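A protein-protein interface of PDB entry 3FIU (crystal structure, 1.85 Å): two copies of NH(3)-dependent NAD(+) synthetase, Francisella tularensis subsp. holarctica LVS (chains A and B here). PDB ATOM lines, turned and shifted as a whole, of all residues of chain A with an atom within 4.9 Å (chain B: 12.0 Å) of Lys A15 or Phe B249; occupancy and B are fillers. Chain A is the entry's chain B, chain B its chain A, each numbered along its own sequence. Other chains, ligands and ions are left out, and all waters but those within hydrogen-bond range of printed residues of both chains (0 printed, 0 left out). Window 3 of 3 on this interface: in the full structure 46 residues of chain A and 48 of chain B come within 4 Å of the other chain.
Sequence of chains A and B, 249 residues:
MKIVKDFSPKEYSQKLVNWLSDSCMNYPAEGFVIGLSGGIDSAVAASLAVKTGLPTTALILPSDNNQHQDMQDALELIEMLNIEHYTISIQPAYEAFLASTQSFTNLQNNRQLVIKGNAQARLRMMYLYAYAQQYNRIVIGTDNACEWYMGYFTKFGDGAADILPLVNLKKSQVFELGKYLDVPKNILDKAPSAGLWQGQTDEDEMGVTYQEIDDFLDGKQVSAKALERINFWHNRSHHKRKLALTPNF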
ATOM      1  N   GLU A  11      19.324   1.246  19.209  1.00  0.00           N
ATOM      2  CA  GLU A  11      18.698   1.695  20.439  1.00  0.00           C
ATOM      3  C   GLU A  11      17.327   1.057  20.631  1.00  0.00           C
ATOM      4  O   GLU A  11      17.024   0.569  21.732  1.00  0.00           O
ATOM      5  CB  GLU A  11      18.592   3.226  20.466  1.00  0.00           C
ATOM      6  CG  GLU A  11      19.916   3.912  20.781  1.00  0.00           C
ATOM      7  CD  GLU A  11      20.898   3.917  19.603  1.00  0.00           C
ATOM      8  OE1 GLU A  11      20.477   3.656  18.440  1.00  0.00           O
ATOM      9  OE2 GLU A  11      22.102   4.194  19.848  1.00  0.00           O
ATOM     10  N   TYR A  12      16.511   1.058  19.575  1.00  0.00           N
ATOM     11  CA  TYR A  12      15.168   0.472  19.674  1.00  0.00           C
ATOM     12  C   TYR A  12      15.261  -1.035  19.953  1.00  0.00           C
ATOM     13  O   TYR A  12      14.491  -1.564  20.743  1.00  0.00           O
ATOM     14  CB  TYR A  12      14.293   0.754  18.438  1.00  0.00           C
ATOM     15  CG  TYR A  12      12.813   0.537  18.710  1.00  0.00           C
ATOM     16  CD1 TYR A  12      12.017   1.582  19.168  1.00  0.00           C
ATOM     17  CD2 TYR A  12      12.210  -0.722  18.522  1.00  0.00           C
ATOM     18  CE1 TYR A  12      10.662   1.401  19.436  1.00  0.00           C
ATOM     19  CE2 TYR A  12      10.857  -0.918  18.782  1.00  0.00           C
ATOM     20  CZ  TYR A  12      10.084   0.148  19.248  1.00  0.00           C
ATOM     21  OH  TYR A  12       8.732  -0.027  19.528  1.00  0.00           O
ATOM     22  N   SER A  13      16.200  -1.714  19.307  1.00  0.00           N
ATOM     23  CA  SER A  13      16.459  -3.111  19.620  1.00  0.00           C
ATOM     24  C   SER A  13      16.796  -3.363  21.103  1.00  0.00           C
ATOM     25  O   SER A  13      16.249  -4.284  21.716  1.00  0.00           O
ATOM     26  CB  SER A  13      17.518  -3.702  18.698  1.00  0.00           C
ATOM     27  OG  SER A  13      17.765  -5.030  19.095  1.00  0.00           O
ATOM     28  N   GLN A  14      17.678  -2.559  21.687  1.00  0.00           N
ATOM     29  CA  GLN A  14      17.987  -2.717  23.112  1.00  0.00           C
ATOM     30  C   GLN A  14      16.778  -2.456  24.015  1.00  0.00           C
ATOM     31  O   GLN A  14      16.570  -3.165  25.005  1.00  0.00           O
ATOM     32  CB  GLN A  14      19.175  -1.856  23.548  1.00  0.00           C
ATOM     33  CG  GLN A  14      19.667  -2.205  24.978  1.00  0.00           C
ATOM     34  CD  GLN A  14      20.006  -3.707  25.157  1.00  0.00           C
ATOM     35  OE1 GLN A  14      19.391  -4.413  25.968  1.00  0.00           O
ATOM     36  NE2 GLN A  14      20.974  -4.188  24.386  1.00  0.00           N
ATOM     37  N   LYS A  15      15.983  -1.445  23.679  1.00  0.00           N
ATOM     38  CA  LYS A  15      14.770  -1.169  24.457  1.00  0.00           C
ATOM     39  C   LYS A  15      13.783  -2.334  24.410  1.00  0.00           C
ATOM     40  O   LYS A  15      13.161  -2.669  25.434  1.00  0.00           O
ATOM     41  CB  LYS A  15      14.086   0.098  23.968  1.00  0.00           C
ATOM     42  CG  LYS A  15      14.784   1.356  24.434  1.00  0.00           C
ATOM     43  CD  LYS A  15      14.026   2.575  23.955  1.00  0.00           C
ATOM     44  CE  LYS A  15      14.030   3.674  25.016  1.00  0.00           C
ATOM     45  NZ  LYS A  15      12.929   3.466  26.026  1.00  0.00           N
ATOM     46  N   LEU A  16      13.659  -2.951  23.234  1.00  0.00           N
ATOM     47  CA  LEU A  16      12.732  -4.076  23.065  1.00  0.00           C
ATOM     48  C   LEU A  16      13.214  -5.313  23.790  1.00  0.00           C
ATOM     49  O   LEU A  16      12.412  -6.028  24.395  1.00  0.00           O
ATOM     50  CB  LEU A  16      12.546  -4.424  21.583  1.00  0.00           C
ATOM     51  CG  LEU A  16      11.379  -3.781  20.846  1.00  0.00           C
ATOM     52  CD1 LEU A  16      11.379  -4.327  19.398  1.00  0.00           C
ATOM     53  CD2 LEU A  16      10.061  -4.095  21.567  1.00  0.00           C
ATOM     54  N   VAL A  17      14.527  -5.561  23.731  1.00  0.00           N
ATOM     55  CA  VAL A  17      15.120  -6.696  24.420  1.00  0.00           C
ATOM     56  C   VAL A  17      14.846  -6.554  25.907  1.00  0.00           C
ATOM     57  O   VAL A  17      14.330  -7.488  26.540  1.00  0.00           O
ATOM     58  CB  VAL A  17      16.643  -6.871  24.091  1.00  0.00           C
ATOM     59  CG1 VAL A  17      17.268  -7.996  24.955  1.00  0.00           C
ATOM     60  CG2 VAL A  17      16.823  -7.184  22.606  1.00  0.00           C
ATOM     61  N   ASN A  18      15.136  -5.369  26.455  1.00  0.00           N
ATOM     62  CA  ASN A  18      14.894  -5.093  27.873  1.00  0.00           C
ATOM     63  C   ASN A  18      13.415  -5.214  28.252  1.00  0.00           C
ATOM     64  O   ASN A  18      13.091  -5.752  29.305  1.00  0.00           O
ATOM     65  CB  ASN A  18      15.412  -3.691  28.258  1.00  0.00           C
ATOM     66  CG  ASN A  18      16.945  -3.595  28.253  1.00  0.00           C
ATOM     67  OD1 ASN A  18      17.646  -4.564  27.970  1.00  0.00           O
ATOM     68  ND2 ASN A  18      17.459  -2.411  28.559  1.00  0.00           N
ATOM     69  N   TRP A  19      12.527  -4.728  27.380  1.00  0.00           N
ATOM     70  CA  TRP A  19      11.096  -4.783  27.635  1.00  0.00           C
ATOM     71  C   TRP A  19      10.573  -6.220  27.563  1.00  0.00           C
ATOM     72  O   TRP A  19       9.712  -6.597  28.369  1.00  0.00           O
ATOM     73  CB  TRP A  19      10.325  -3.846  26.689  1.00  0.00           C
ATOM     74  CG  TRP A  19       8.808  -3.996  26.780  1.00  0.00           C
ATOM     75  CD1 TRP A  19       7.968  -3.437  27.700  1.00  0.00           C
ATOM     76  CD2 TRP A  19       7.987  -4.795  25.921  1.00  0.00           C
ATOM     77  NE1 TRP A  19       6.658  -3.808  27.440  1.00  0.00           N
ATOM     78  CE2 TRP A  19       6.654  -4.658  26.361  1.00  0.00           C
ATOM     79  CE3 TRP A  19       8.256  -5.604  24.811  1.00  0.00           C
ATOM     80  CZ2 TRP A  19       5.594  -5.308  25.734  1.00  0.00           C
ATOM     81  CZ3 TRP A  19       7.203  -6.244  24.185  1.00  0.00           C
ATOM     82  CH2 TRP A  19       5.891  -6.087  24.641  1.00  0.00           C
ATOM     83  N   ASN A 168       4.261  -1.654  17.252  1.00  0.00           N
ATOM     84  CA  ASN A 168       4.422  -0.203  16.990  1.00  0.00           C
ATOM     85  C   ASN A 168       5.342   0.110  15.801  1.00  0.00           C
ATOM     86  O   ASN A 168       5.485   1.271  15.419  1.00  0.00           O
ATOM     87  CB  ASN A 168       4.942   0.541  18.231  1.00  0.00           C
ATOM     88  CG  ASN A 168       4.020   0.410  19.428  1.00  0.00           C
ATOM     89  OD1 ASN A 168       4.482   0.321  20.570  1.00  0.00           O
ATOM     90  ND2 ASN A 168       2.727   0.370  19.178  1.00  0.00           N
ATOM     91  N   ALA B 244      -3.016  -8.802  24.557  1.00  0.00           N
ATOM     92  CA  ALA B 244      -1.579  -9.054  24.620  1.00  0.00           C
ATOM     93  C   ALA B 244      -0.806  -7.804  25.048  1.00  0.00           C
ATOM     94  O   ALA B 244      -1.200  -6.662  24.690  1.00  0.00           O
ATOM     95  CB  ALA B 244      -1.093  -9.540  23.260  1.00  0.00           C
ATOM     96  N   LEU B 245       0.289  -8.023  25.787  1.00  0.00           N
ATOM     97  CA  LEU B 245       1.211  -6.939  26.211  1.00  0.00           C
ATOM     98  C   LEU B 245       1.834  -6.250  25.011  1.00  0.00           C
ATOM     99  O   LEU B 245       2.255  -6.909  24.048  1.00  0.00           O
ATOM    100  CB  LEU B 245       2.317  -7.463  27.132  1.00  0.00           C
ATOM    101  CG  LEU B 245       1.856  -8.203  28.411  1.00  0.00           C
ATOM    102  CD1 LEU B 245       3.039  -8.838  29.185  1.00  0.00           C
ATOM    103  CD2 LEU B 245       1.014  -7.302  29.314  1.00  0.00           C
ATOM    104  N   THR B 246       1.869  -4.924  25.042  1.00  0.00           N
ATOM    105  CA  THR B 246       2.494  -4.161  23.961  1.00  0.00           C
ATOM    106  C   THR B 246       3.450  -3.121  24.563  1.00  0.00           C
ATOM    107  O   THR B 246       3.252  -2.689  25.707  1.00  0.00           O
ATOM    108  CB  THR B 246       1.457  -3.462  23.022  1.00  0.00           C
ATOM    109  OG1 THR B 246       0.763  -2.412  23.722  1.00  0.00           O
ATOM    110  CG2 THR B 246       0.435  -4.458  22.490  1.00  0.00           C
ATOM    111  N   PRO B 247       4.496  -2.732  23.809  1.00  0.00           N
ATOM    112  CA  PRO B 247       5.413  -1.723  24.327  1.00  0.00           C
ATOM    113  C   PRO B 247       4.677  -0.373  24.352  1.00  0.00           C
ATOM    114  O   PRO B 247       3.823  -0.114  23.501  1.00  0.00           O
ATOM    115  CB  PRO B 247       6.529  -1.661  23.274  1.00  0.00           C
ATOM    116  CG  PRO B 247       6.301  -2.829  22.367  1.00  0.00           C
ATOM    117  CD  PRO B 247       4.857  -3.164  22.447  1.00  0.00           C
ATOM    118  N   ASN B 248       5.023   0.472  25.302  1.00  0.00           N
ATOM    119  CA  ASN B 248       4.556   1.866  25.296  1.00  0.00           C
ATOM    120  C   ASN B 248       5.537   2.799  24.558  1.00  0.00           C
ATOM    121  O   ASN B 248       5.526   4.015  24.781  1.00  0.00           O
ATOM    122  CB  ASN B 248       4.377   2.352  26.737  1.00  0.00           C
ATOM    123  CG  ASN B 248       5.727   2.469  27.498  1.00  0.00           C
ATOM    124  OD1 ASN B 248       6.684   1.727  27.230  1.00  0.00           O
ATOM    125  ND2 ASN B 248       5.790   3.404  28.448  1.00  0.00           N
ATOM    126  N   PHE B 249       6.396   2.236  23.709  1.00  0.00           N
ATOM    127  CA  PHE B 249       7.394   3.026  22.999  1.00  0.00           C
ATOM    128  C   PHE B 249       7.577   2.562  21.545  1.00  0.00           C
ATOM    129  O   PHE B 249       8.164   3.312  20.765  1.00  0.00           O
ATOM    130  CB  PHE B 249       8.747   3.033  23.755  1.00  0.00           C
ATOM    131  CG  PHE B 249       9.324   1.658  23.970  1.00  0.00           C
ATOM    132  CD1 PHE B 249      10.078   1.039  22.972  1.00  0.00           C
ATOM    133  CD2 PHE B 249       9.089   0.966  25.165  1.00  0.00           C
ATOM    134  CE1 PHE B 249      10.580  -0.250  23.160  1.00  0.00           C
ATOM    135  CE2 PHE B 249       9.591  -0.309  25.362  1.00  0.00           C
ATOM    136  CZ  PHE B 249      10.334  -0.923  24.366  1.00  0.00           C
ATOM    137  OXT PHE B 249       7.178   1.475  21.106  1.00  0.00           O
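The backbone carbonyl oxygen of Pro B247 lies close to the side-chain amide oxygen of Asn A168. The chain-end carboxylate (OXT) of Phe B249 sits at hydrogen-bond distance from the side-chain hydroxyl (OH) of Tyr A12 (2.7 Å). The side-chain amide oxygen (OD1) of Asn A168 sits close to the chain-end carboxylate (OXT) of Phe B249 (3.0 Å).
Among the printed residues, merely in contact across the chains: Lys A15 with Phe B249 (3.5 Å), Trp A19 with Leu B245 (3.8 Å), Trp A19 with Thr B246 (3.3 Å), Trp A19 with Pro B247 (3.4 Å) and Trp A19 with Phe B249 (3.7 Å).
Lys A15 touches one residue of chain B. Of chain A, only Tyr A12 (2.7 Å), Lys A15 (3.5 Å), Trp A19 (3.7 Å) and Asn A168 (3.0 Å) come within 4 Å of Phe B249. Tyr A12 touches just one residue of chain B: Phe B249 (2.7 Å). Ser A13 touches none of the printed residues of chain B. No residue of chain B comes within 4 Å of Gln A14. No residue of chain B comes within 4 Å of Leu A16. Of chain B, only Leu B245, Thr B246, Pro B247 and Phe B249 come within 4 Å of Trp A19. Of chain B, only Pro B247 (3.0 Å) and Phe B249 (3.0 Å) come within 4 Å of Asn A168. Of the printed residues of chain A, Leu B245 touches Trp A19 (3.8 Å). Of the printed residues of chain A, Pro B247 touches Trp A19 (3.4 Å) and Asn A168 (3.0 Å). Of the printed residues of chain A, Thr B246 touches Trp A19 (3.3 Å). Asn B248 touches none of the printed residues of chain A. Glu A11 touches none of the printed residues of chain B. The nearest residue of chain B that does not touch Lys A15 is Asn B248 (6.6 Å). The nearest printed residue of chain A that does not touch Thr B246 is Asn A168 (5.4 Å).
Of the 10 printed residues of chain A, 4 touch a printed residue of chain B. Hydrophobic or aromatic side chains of chain A within 4 Å of the printed part of chain B: Tyr A12 and Trp A19. Of the 6 printed residues of chain B, 4 touch a printed residue of chain A. Hydrophobic or aromatic side chains of chain B that line the printed part of chain A: Pro B247 and Phe B249.
No position is printed for both chains. Of the 8 pairs that touch across the chains among the printed residues, none has its exchanged pair printed and touching as well.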
